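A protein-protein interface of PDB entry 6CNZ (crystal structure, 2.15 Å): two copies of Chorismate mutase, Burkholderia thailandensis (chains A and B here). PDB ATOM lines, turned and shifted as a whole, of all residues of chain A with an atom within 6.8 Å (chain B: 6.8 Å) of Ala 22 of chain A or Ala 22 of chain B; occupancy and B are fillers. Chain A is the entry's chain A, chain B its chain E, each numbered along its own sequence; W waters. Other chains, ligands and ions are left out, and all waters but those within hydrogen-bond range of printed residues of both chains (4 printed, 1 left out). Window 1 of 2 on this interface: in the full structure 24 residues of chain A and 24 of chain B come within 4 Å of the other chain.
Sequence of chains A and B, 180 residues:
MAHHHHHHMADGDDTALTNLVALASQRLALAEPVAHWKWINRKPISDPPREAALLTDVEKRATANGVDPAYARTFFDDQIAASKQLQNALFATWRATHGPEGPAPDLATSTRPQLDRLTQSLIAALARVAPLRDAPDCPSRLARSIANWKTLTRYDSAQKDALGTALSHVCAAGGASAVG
Thr 18 of chain B touches its own counterpart, Thr 18 of chain A.
Thr 18 of chain A touches Asn 19 of chain B, and with the chains exchanged Asn 19 of chain A touches Thr 18 of chain B.
Leu 23 of chain A touches Trp 149 of chain B, and with the chains exchanged Trp 149 of chain A touches Leu 23 of chain B.
Trp 149 of chain A touches Gln 26 of chain B, but with the chains exchanged Gln 26 of chain A does not touch Trp 149 of chain B (4.1 Å).
15 positions are printed for both chains.
Of the 9 pairs that touch across the chains among the printed residues, 8 have their exchanged pair printed and touching as well.
Ala 22 of chain A touches just one residue of chain B: Ala 22.
Printed residues of chain A within 4 Å of Ala 22 of chain B: Ala 22 (3.9 Å).
Of the printed residues of chain B, Asn 19 of chain A touches Thr 18 (3.1 Å) and Trp 149 (3.3 Å).
Printed residues of chain A within 4 Å of Thr 18 of chain B: Thr 18 (3.9 Å) and Asn 19 (3.1 Å).
Printed residues of chain B within 4 Å of Trp 149 of chain A: Asn 19 (3.5 Å), Leu 23 (3.5 Å) and Gln 26 (3.7 Å).
Leu 163 of chain B touches none of the printed residues of chain A.
Ser 25 of chain A touches none of the printed residues of chain B.
The nearest residue of chain A that does not touch Ala 22 of chain B is Trp 149 of chain A (4.7 Å).
Of the 15 printed residues of chain B, 6 touch a printed residue of chain A.
Printed residues of chain B that touch a printed residue of chain A: Thr 18, Asn 19, Ala 22, Leu 23, Gln 26 and Trp 149.
Hydrophobic or aromatic side chains of chain B within 4 Å of the printed part of chain A: Ala 22, Leu 23 and Trp 149.
OG of Ser 25 of chain A sits at hydrogen-bond distance from NE1 of Trp 149 of chain A (2.9 Å).
The side-chain hydroxyl of Ser 25 of chain B sits at hydrogen-bond distance from the indole nitrogen of Trp 149 of chain B (3.0 Å).
Water W3 bridges the backbone carbonyl oxygen (O) of Thr 18 of chain A and the side-chain amide oxygen (OD1) of Asn 19 of chain B.
Water W4 lies within hydrogen-bond range of the side-chain hydroxyl (OG) of Ser 25 of chain B, the side-chain amide nitrogen (NE2) of Gln 26 of chain A and the backbone NH (N) of Gln 26 of chain B.
Water W1 lies within hydrogen-bond range of the side-chain amide oxygen (OD1) of Asn 19 of chain A and the backbone carbonyl oxygen (O) of Thr 18 of chain B.
Water W2 lies within hydrogen-bond range of OG of Ser 25 of chain A (2.8 Å) and NE2 of Gln 26 of chain B (3.1 Å).
Among the printed residues, merely in contact across the chains: Asn 19 of chain A with Thr 18 of chain B, Thr 18 of chain A with Asn 19 of chain B, Asn 19 of chain A with Trp 149 of chain B, Trp 149 of chain A with Asn 19 of chain B, Trp 149 of chain A with Leu 23 of chain B, Leu 23 of chain A with Trp 149 of chain B, Trp 149 of chain A with Gln 26 of chain B, Ala 22 of chain A with Ala 22 of chain B and Thr 18 of chain A with Thr 18 of chain B.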
ATOM      1  N   LEU A  17      -9.119   8.076 -20.927  1.00  0.00           N
ATOM      2  CA  LEU A  17      -8.547   6.861 -20.362  1.00  0.00           C
ATOM      3  C   LEU A  17      -9.031   6.622 -18.939  1.00  0.00           C
ATOM      4  O   LEU A  17      -9.360   5.490 -18.574  1.00  0.00           O
ATOM      5  CB  LEU A  17      -7.021   6.941 -20.379  1.00  0.00           C
ATOM      6  CG  LEU A  17      -6.330   6.830 -21.727  1.00  0.00           C
ATOM      7  CD1 LEU A  17      -4.830   7.061 -21.523  1.00  0.00           C
ATOM      8  CD2 LEU A  17      -6.593   5.466 -22.307  1.00  0.00           C
ATOM      9  N   THR A  18      -9.048   7.673 -18.113  1.00  0.00           N
ATOM     10  CA  THR A  18      -9.457   7.536 -16.719  1.00  0.00           C
ATOM     11  C   THR A  18     -10.875   6.997 -16.604  1.00  0.00           C
ATOM     12  O   THR A  18     -11.159   6.127 -15.767  1.00  0.00           O
ATOM     13  CB  THR A  18      -9.351   8.897 -16.027  1.00  0.00           C
ATOM     14  OG1 THR A  18      -8.069   9.474 -16.293  1.00  0.00           O
ATOM     15  CG2 THR A  18      -9.524   8.741 -14.523  1.00  0.00           C
ATOM     16  N   ASN A  19     -11.785   7.508 -17.434  1.00  0.00           N
ATOM     17  CA  ASN A  19     -13.164   7.028 -17.415  1.00  0.00           C
ATOM     18  C   ASN A  19     -13.248   5.586 -17.886  1.00  0.00           C
ATOM     19  O   ASN A  19     -14.004   4.783 -17.319  1.00  0.00           O
ATOM     20  CB  ASN A  19     -14.034   7.935 -18.275  1.00  0.00           C
ATOM     21  CG  ASN A  19     -14.596   9.112 -17.489  1.00  0.00           C
ATOM     22  OD1 ASN A  19     -14.701   9.054 -16.266  1.00  0.00           O
ATOM     23  ND2 ASN A  19     -14.993  10.160 -18.189  1.00  0.00           N
ATOM     24  N   LEU A  20     -12.443   5.234 -18.892  1.00  0.00           N
ATOM     25  CA  LEU A  20     -12.414   3.861 -19.394  1.00  0.00           C
ATOM     26  C   LEU A  20     -11.970   2.882 -18.306  1.00  0.00           C
ATOM     27  O   LEU A  20     -12.585   1.827 -18.113  1.00  0.00           O
ATOM     28  CB  LEU A  20     -11.478   3.771 -20.611  1.00  0.00           C
ATOM     29  CG  LEU A  20     -11.493   2.440 -21.359  1.00  0.00           C
ATOM     30  CD1 LEU A  20     -12.898   2.176 -21.905  1.00  0.00           C
ATOM     31  CD2 LEU A  20     -10.472   2.419 -22.483  1.00  0.00           C
ATOM     32  N   VAL A  21     -10.883   3.210 -17.599  1.00  0.00           N
ATOM     33  CA  VAL A  21     -10.412   2.376 -16.490  1.00  0.00           C
ATOM     34  C   VAL A  21     -11.513   2.193 -15.445  1.00  0.00           C
ATOM     35  O   VAL A  21     -11.803   1.076 -15.004  1.00  0.00           O
ATOM     36  CB  VAL A  21      -9.140   2.999 -15.874  1.00  0.00           C
ATOM     37  CG1 VAL A  21      -8.686   2.236 -14.611  1.00  0.00           C
ATOM     38  CG2 VAL A  21      -8.031   3.038 -16.898  1.00  0.00           C
ATOM     39  N   ALA A  22     -12.135   3.294 -15.027  1.00  0.00           N
ATOM     40  CA  ALA A  22     -13.151   3.214 -13.978  1.00  0.00           C
ATOM     41  C   ALA A  22     -14.297   2.304 -14.386  1.00  0.00           C
ATOM     42  O   ALA A  22     -14.766   1.483 -13.588  1.00  0.00           O
ATOM     43  CB  ALA A  22     -13.678   4.610 -13.647  1.00  0.00           C
ATOM     44  N   LEU A  23     -14.741   2.409 -15.639  1.00  0.00           N
ATOM     45  CA  LEU A  23     -15.874   1.594 -16.062  1.00  0.00           C
ATOM     46  C   LEU A  23     -15.468   0.136 -16.226  1.00  0.00           C
ATOM     47  O   LEU A  23     -16.240  -0.772 -15.870  1.00  0.00           O
ATOM     48  CB  LEU A  23     -16.478   2.156 -17.350  1.00  0.00           C
ATOM     49  CG  LEU A  23     -17.241   3.484 -17.166  1.00  0.00           C
ATOM     50  CD1 LEU A  23     -17.414   4.190 -18.512  1.00  0.00           C
ATOM     51  CD2 LEU A  23     -18.603   3.292 -16.441  1.00  0.00           C
ATOM     52  N   ALA A  24     -14.253  -0.113 -16.742  1.00  0.00           N
ATOM     53  CA  ALA A  24     -13.780  -1.487 -16.867  1.00  0.00           C
ATOM     54  C   ALA A  24     -13.682  -2.137 -15.501  1.00  0.00           C
ATOM     55  O   ALA A  24     -14.015  -3.313 -15.335  1.00  0.00           O
ATOM     56  CB  ALA A  24     -12.420  -1.541 -17.571  1.00  0.00           C
ATOM     57  N   SER A  25     -13.220  -1.381 -14.512  1.00  0.00           N
ATOM     58  CA  SER A  25     -13.147  -1.912 -13.158  1.00  0.00           C
ATOM     59  C   SER A  25     -14.542  -2.150 -12.592  1.00  0.00           C
ATOM     60  O   SER A  25     -14.787  -3.154 -11.912  1.00  0.00           O
ATOM     61  CB  SER A  25     -12.347  -0.940 -12.277  1.00  0.00           C
ATOM     62  OG  SER A  25     -12.456  -1.274 -10.908  1.00  0.00           O
ATOM     63  N   GLN A  26     -15.467  -1.233 -12.874  1.00  0.00           N
ATOM     64  CA  GLN A  26     -16.841  -1.394 -12.425  1.00  0.00           C
ATOM     65  C   GLN A  26     -17.460  -2.662 -13.009  1.00  0.00           C
ATOM     66  O   GLN A  26     -18.115  -3.430 -12.295  1.00  0.00           O
ATOM     67  CB  GLN A  26     -17.644  -0.143 -12.806  1.00  0.00           C
ATOM     68  CG  GLN A  26     -19.046  -0.070 -12.241  1.00  0.00           C
ATOM     69  CD  GLN A  26     -19.742   1.284 -12.495  1.00  0.00           C
ATOM     70  OE1 GLN A  26     -19.097   2.305 -12.729  1.00  0.00           O
ATOM     71  NE2 GLN A  26     -21.064   1.277 -12.443  1.00  0.00           N
ATOM     72  N   ARG A  27     -17.231  -2.920 -14.293  1.00  0.00           N
ATOM     73  CA  ARG A  27     -17.766  -4.144 -14.891  1.00  0.00           C
ATOM     74  C   ARG A  27     -17.115  -5.379 -14.288  1.00  0.00           C
ATOM     75  O   ARG A  27     -17.796  -6.367 -13.978  1.00  0.00           O
ATOM     76  CB  ARG A  27     -17.565  -4.128 -16.406  1.00  0.00           C
ATOM     77  CG  ARG A  27     -18.371  -5.186 -17.140  1.00  0.00           C
ATOM     78  CD  ARG A  27     -17.868  -5.363 -18.568  1.00  0.00           C
ATOM     79  NE  ARG A  27     -18.815  -6.124 -19.364  1.00  0.00           N
ATOM     80  CZ  ARG A  27     -18.855  -7.448 -19.401  1.00  0.00           C
ATOM     81  NH1 ARG A  27     -17.977  -8.161 -18.702  1.00  0.00           N
ATOM     82  NH2 ARG A  27     -19.775  -8.054 -20.141  1.00  0.00           N
ATOM     83  N   LEU A 118     -23.403  -1.491 -18.648  1.00  0.00           N
ATOM     84  CA  LEU A 118     -21.997  -1.139 -18.823  1.00  0.00           C
ATOM     85  C   LEU A 118     -21.532  -1.353 -20.261  1.00  0.00           C
ATOM     86  O   LEU A 118     -20.587  -0.690 -20.711  1.00  0.00           O
ATOM     87  CB  LEU A 118     -21.131  -1.921 -17.838  1.00  0.00           C
ATOM     88  CG  LEU A 118     -21.205  -1.289 -16.440  1.00  0.00           C
ATOM     89  CD1 LEU A 118     -20.725  -2.250 -15.368  1.00  0.00           C
ATOM     90  CD2 LEU A 118     -20.439   0.008 -16.371  1.00  0.00           C
ATOM     91  N   LEU A 122     -19.218   1.420 -21.744  1.00  0.00           N
ATOM     92  CA  LEU A 122     -17.885   1.042 -22.198  1.00  0.00           C
ATOM     93  C   LEU A 122     -17.690   1.353 -23.671  1.00  0.00           C
ATOM     94  O   LEU A 122     -16.618   1.825 -24.072  1.00  0.00           O
ATOM     95  CB  LEU A 122     -17.655  -0.440 -21.935  1.00  0.00           C
ATOM     96  CG  LEU A 122     -17.337  -0.707 -20.464  1.00  0.00           C
ATOM     97  CD1 LEU A 122     -17.221  -2.203 -20.209  1.00  0.00           C
ATOM     98  CD2 LEU A 122     -16.036   0.001 -20.088  1.00  0.00           C
ATOM     99  N   TRP A 149      -5.756   4.210 -10.378  1.00  0.00           N
ATOM    100  CA  TRP A 149      -7.021   3.630  -9.951  1.00  0.00           C
ATOM    101  C   TRP A 149      -6.797   2.512  -8.949  1.00  0.00           C
ATOM    102  O   TRP A 149      -7.525   2.407  -7.959  1.00  0.00           O
ATOM    103  CB  TRP A 149      -7.788   3.117 -11.170  1.00  0.00           C
ATOM    104  CG  TRP A 149      -9.056   2.444 -10.836  1.00  0.00           C
ATOM    105  CD1 TRP A 149      -9.257   1.102 -10.707  1.00  0.00           C
ATOM    106  CD2 TRP A 149     -10.322   3.068 -10.586  1.00  0.00           C
ATOM    107  NE1 TRP A 149     -10.563   0.852 -10.398  1.00  0.00           N
ATOM    108  CE2 TRP A 149     -11.246   2.038 -10.327  1.00  0.00           C
ATOM    109  CE3 TRP A 149     -10.765   4.395 -10.561  1.00  0.00           C
ATOM    110  CZ2 TRP A 149     -12.593   2.291 -10.040  1.00  0.00           C
ATOM    111  CZ3 TRP A 149     -12.109   4.649 -10.284  1.00  0.00           C
ATOM    112  CH2 TRP A 149     -13.006   3.597 -10.032  1.00  0.00           C
ATOM    113  N   LEU A 163      -7.894  -6.887 -14.123  1.00  0.00           N
ATOM    114  CA  LEU A 163      -8.094  -5.570 -14.728  1.00  0.00           C
ATOM    115  C   LEU A 163      -7.029  -5.294 -15.780  1.00  0.00           C
ATOM    116  O   LEU A 163      -7.323  -4.678 -16.812  1.00  0.00           O
ATOM    117  CB  LEU A 163      -8.086  -4.472 -13.662  1.00  0.00           C
ATOM    118  CG  LEU A 163      -8.232  -2.994 -14.064  1.00  0.00           C
ATOM    119  CD1 LEU A 163      -9.572  -2.707 -14.703  1.00  0.00           C
ATOM    120  CD2 LEU A 163      -8.042  -2.093 -12.851  1.00  0.00           C
ATOM    121  N   LEU A 167      -7.703  -4.469 -19.937  1.00  0.00           N
ATOM    122  CA  LEU A 167      -7.245  -3.270 -20.626  1.00  0.00           C
ATOM    123  C   LEU A 167      -6.033  -3.546 -21.512  1.00  0.00           C
ATOM    124  O   LEU A 167      -5.282  -2.626 -21.839  1.00  0.00           O
ATOM    125  CB  LEU A 167      -6.945  -2.179 -19.602  1.00  0.00           C
ATOM    126  CG  LEU A 167      -8.191  -1.852 -18.749  1.00  0.00           C
ATOM    127  CD1 LEU A 167      -7.861  -1.035 -17.501  1.00  0.00           C
ATOM    128  CD2 LEU A 167      -9.229  -1.133 -19.611  1.00  0.00           C
ATOM    129  N   LEU B  17     -10.338  14.789 -10.409  1.00  0.00           N
ATOM    130  CA  LEU B  17     -11.768  15.071 -10.419  1.00  0.00           C
ATOM    131  C   LEU B  17     -12.536  13.939 -11.080  1.00  0.00           C
ATOM    132  O   LEU B  17     -13.576  13.498 -10.569  1.00  0.00           O
ATOM    133  CB  LEU B  17     -12.035  16.389 -11.139  1.00  0.00           C
ATOM    134  CG  LEU B  17     -11.520  17.611 -10.389  1.00  0.00           C
ATOM    135  CD1 LEU B  17     -11.689  18.852 -11.232  1.00  0.00           C
ATOM    136  CD2 LEU B  17     -12.259  17.736  -9.059  1.00  0.00           C
ATOM    137  N   THR B  18     -12.027  13.444 -12.210  1.00  0.00           N
ATOM    138  CA  THR B  18     -12.728  12.386 -12.923  1.00  0.00           C
ATOM    139  C   THR B  18     -12.903  11.156 -12.041  1.00  0.00           C
ATOM    140  O   THR B  18     -13.996  10.592 -11.961  1.00  0.00           O
ATOM    141  CB  THR B  18     -11.983  12.040 -14.209  1.00  0.00           C
ATOM    142  OG1 THR B  18     -11.924  13.201 -15.044  1.00  0.00           O
ATOM    143  CG2 THR B  18     -12.727  10.976 -14.948  1.00  0.00           C
ATOM    144  N   ASN B  19     -11.851  10.763 -11.326  1.00  0.00           N
ATOM    145  CA  ASN B  19     -11.961   9.603 -10.452  1.00  0.00           C
ATOM    146  C   ASN B  19     -12.943   9.859  -9.311  1.00  0.00           C
ATOM    147  O   ASN B  19     -13.737   8.974  -8.968  1.00  0.00           O
ATOM    148  CB  ASN B  19     -10.582   9.214  -9.922  1.00  0.00           C
ATOM    149  CG  ASN B  19      -9.821   8.345 -10.899  1.00  0.00           C
ATOM    150  OD1 ASN B  19     -10.418   7.682 -11.750  1.00  0.00           O
ATOM    151  ND2 ASN B  19      -8.503   8.315 -10.767  1.00  0.00           N
ATOM    152  N   LEU B  20     -12.925  11.065  -8.725  1.00  0.00           N
ATOM    153  CA  LEU B  20     -13.880  11.378  -7.656  1.00  0.00           C
ATOM    154  C   LEU B  20     -15.321  11.292  -8.156  1.00  0.00           C
ATOM    155  O   LEU B  20     -16.199  10.766  -7.459  1.00  0.00           O
ATOM    156  CB  LEU B  20     -13.593  12.765  -7.070  1.00  0.00           C
ATOM    157  CG  LEU B  20     -14.385  13.187  -5.822  1.00  0.00           C
ATOM    158  CD1 LEU B  20     -14.050  12.298  -4.643  1.00  0.00           C
ATOM    159  CD2 LEU B  20     -14.131  14.654  -5.454  1.00  0.00           C
ATOM    160  N   VAL B  21     -15.578  11.791  -9.367  1.00  0.00           N
ATOM    161  CA  VAL B  21     -16.918  11.717  -9.943  1.00  0.00           C
ATOM    162  C   VAL B  21     -17.341  10.262 -10.117  1.00  0.00           C
ATOM    163  O   VAL B  21     -18.441   9.861  -9.721  1.00  0.00           O
ATOM    164  CB  VAL B  21     -16.967  12.472 -11.283  1.00  0.00           C
ATOM    165  CG1 VAL B  21     -18.236  12.097 -12.054  1.00  0.00           C
ATOM    166  CG2 VAL B  21     -16.878  13.983 -11.056  1.00  0.00           C
ATOM    167  N   ALA B  22     -16.466   9.456 -10.723  1.00  0.00           N
ATOM    168  CA  ALA B  22     -16.780   8.056 -10.983  1.00  0.00           C
ATOM    169  C   ALA B  22     -17.109   7.315  -9.693  1.00  0.00           C
ATOM    170  O   ALA B  22     -18.082   6.549  -9.624  1.00  0.00           O
ATOM    171  CB  ALA B  22     -15.605   7.392 -11.701  1.00  0.00           C
ATOM    172  N   LEU B  23     -16.302   7.527  -8.656  1.00  0.00           N
ATOM    173  CA  LEU B  23     -16.525   6.799  -7.415  1.00  0.00           C
ATOM    174  C   LEU B  23     -17.779   7.297  -6.689  1.00  0.00           C
ATOM    175  O   LEU B  23     -18.434   6.522  -5.981  1.00  0.00           O
ATOM    176  CB  LEU B  23     -15.276   6.904  -6.531  1.00  0.00           C
ATOM    177  CG  LEU B  23     -14.036   6.113  -6.974  1.00  0.00           C
ATOM    178  CD1 LEU B  23     -12.829   6.478  -6.129  1.00  0.00           C
ATOM    179  CD2 LEU B  23     -14.284   4.599  -6.897  1.00  0.00           C
ATOM    180  N   ALA B  24     -18.127   8.577  -6.839  1.00  0.00           N
ATOM    181  CA  ALA B  24     -19.378   9.053  -6.247  1.00  0.00           C
ATOM    182  C   ALA B  24     -20.574   8.417  -6.945  1.00  0.00           C
ATOM    183  O   ALA B  24     -21.533   7.987  -6.289  1.00  0.00           O
ATOM    184  CB  ALA B  24     -19.467  10.580  -6.322  1.00  0.00           C
ATOM    185  N   SER B  25     -20.531   8.350  -8.280  1.00  0.00           N
ATOM    186  CA  SER B  25     -21.587   7.672  -9.025  1.00  0.00           C
ATOM    187  C   SER B  25     -21.690   6.212  -8.602  1.00  0.00           C
ATOM    188  O   SER B  25     -22.783   5.706  -8.345  1.00  0.00           O
ATOM    189  CB  SER B  25     -21.323   7.800 -10.522  1.00  0.00           C
ATOM    190  OG  SER B  25     -22.279   7.110 -11.310  1.00  0.00           O
ATOM    191  N   GLN B  26     -20.552   5.529  -8.506  1.00  0.00           N
ATOM    192  CA  GLN B  26     -20.536   4.137  -8.066  1.00  0.00           C
ATOM    193  C   GLN B  26     -21.242   3.962  -6.720  1.00  0.00           C
ATOM    194  O   GLN B  26     -22.022   3.026  -6.532  1.00  0.00           O
ATOM    195  CB  GLN B  26     -19.084   3.662  -7.969  1.00  0.00           C
ATOM    196  CG  GLN B  26     -18.775   2.350  -8.627  1.00  0.00           C
ATOM    197  CD  GLN B  26     -17.265   2.084  -8.694  1.00  0.00           C
ATOM    198  OE1 GLN B  26     -16.519   2.810  -9.352  1.00  0.00           O
ATOM    199  NE2 GLN B  26     -16.821   1.044  -8.014  1.00  0.00           N
ATOM    200  N   ARG B  27     -20.944   4.827  -5.750  1.00  0.00           N
ATOM    201  CA  ARG B  27     -21.582   4.679  -4.449  1.00  0.00           C
ATOM    202  C   ARG B  27     -23.077   4.928  -4.554  1.00  0.00           C
ATOM    203  O   ARG B  27     -23.875   4.203  -3.960  1.00  0.00           O
ATOM    204  CB  ARG B  27     -20.954   5.621  -3.423  1.00  0.00           C
ATOM    205  CG  ARG B  27     -21.441   5.340  -2.013  1.00  0.00           C
ATOM    206  CD  ARG B  27     -21.108   6.492  -1.088  1.00  0.00           C
ATOM    207  NE  ARG B  27     -21.077   6.051   0.295  1.00  0.00           N
ATOM    208  CZ  ARG B  27     -22.115   6.120   1.118  1.00  0.00           C
ATOM    209  NH1 ARG B  27     -23.273   6.633   0.698  1.00  0.00           N
ATOM    210  NH2 ARG B  27     -21.986   5.686   2.362  1.00  0.00           N
ATOM    211  N   LEU B 122     -13.216   6.688  -1.578  1.00  0.00           N
ATOM    212  CA  LEU B 122     -13.595   8.086  -1.719  1.00  0.00           C
ATOM    213  C   LEU B 122     -12.709   8.990  -0.878  1.00  0.00           C
ATOM    214  O   LEU B 122     -12.406  10.119  -1.283  1.00  0.00           O
ATOM    215  CB  LEU B 122     -15.048   8.260  -1.315  1.00  0.00           C
ATOM    216  CG  LEU B 122     -16.049   7.874  -2.387  1.00  0.00           C
ATOM    217  CD1 LEU B 122     -17.426   7.816  -1.757  1.00  0.00           C
ATOM    218  CD2 LEU B 122     -15.991   8.886  -3.538  1.00  0.00           C
ATOM    219  N   TRP B 149     -18.940  12.383 -17.569  1.00  0.00           N
ATOM    220  CA  TRP B 149     -19.374  11.123 -16.984  1.00  0.00           C
ATOM    221  C   TRP B 149     -20.830  10.827 -17.324  1.00  0.00           C
ATOM    222  O   TRP B 149     -21.157   9.717 -17.758  1.00  0.00           O
ATOM    223  CB  TRP B 149     -19.152  11.160 -15.467  1.00  0.00           C
ATOM    224  CG  TRP B 149     -19.598   9.919 -14.756  1.00  0.00           C
ATOM    225  CD1 TRP B 149     -20.748   9.758 -14.032  1.00  0.00           C
ATOM    226  CD2 TRP B 149     -18.909   8.664 -14.692  1.00  0.00           C
ATOM    227  NE1 TRP B 149     -20.821   8.474 -13.532  1.00  0.00           N
ATOM    228  CE2 TRP B 149     -19.707   7.784 -13.924  1.00  0.00           C
ATOM    229  CE3 TRP B 149     -17.720   8.188 -15.226  1.00  0.00           C
ATOM    230  CZ2 TRP B 149     -19.333   6.479 -13.666  1.00  0.00           C
ATOM    231  CZ3 TRP B 149     -17.346   6.888 -14.959  1.00  0.00           C
ATOM    232  CH2 TRP B 149     -18.148   6.051 -14.182  1.00  0.00           C
ATOM    233  N   LEU B 163     -26.489  12.784  -7.879  1.00  0.00           N
ATOM    234  CA  LEU B 163     -25.061  12.968  -8.134  1.00  0.00           C
ATOM    235  C   LEU B 163     -24.653  14.421  -7.925  1.00  0.00           C
ATOM    236  O   LEU B 163     -23.594  14.699  -7.352  1.00  0.00           O
ATOM    237  CB  LEU B 163     -24.701  12.507  -9.544  1.00  0.00           C
ATOM    238  CG  LEU B 163     -23.192  12.483  -9.756  1.00  0.00           C
ATOM    239  CD1 LEU B 163     -22.588  11.420  -8.863  1.00  0.00           C
ATOM    240  CD2 LEU B 163     -22.848  12.223 -11.206  1.00  0.00           C
ATOM    241  N   LEU B 167     -21.835  15.936  -5.153  1.00  0.00           N
ATOM    242  CA  LEU B 167     -20.631  16.644  -5.564  1.00  0.00           C
ATOM    243  C   LEU B 167     -20.734  18.150  -5.332  1.00  0.00           C
ATOM    244  O   LEU B 167     -19.913  18.910  -5.860  1.00  0.00           O
ATOM    245  CB  LEU B 167     -20.326  16.338  -7.032  1.00  0.00           C
ATOM    246  CG  LEU B 167     -20.123  14.853  -7.366  1.00  0.00           C
ATOM    247  CD1 LEU B 167     -20.018  14.607  -8.897  1.00  0.00           C
ATOM    248  CD2 LEU B 167     -18.899  14.312  -6.633  1.00  0.00           C
HETATM  249  O   HOH W   1     -15.706  10.552 -14.172  1.00  0.00           O
HETATM  250  O   HOH W   2     -14.754  -0.843  -9.289  1.00  0.00           O
HETATM  251  O   HOH W   3      -9.794   5.621 -13.534  1.00  0.00           O
HETATM  252  O   HOH W   4     -21.697   4.477 -11.542  1.00  0.00           O
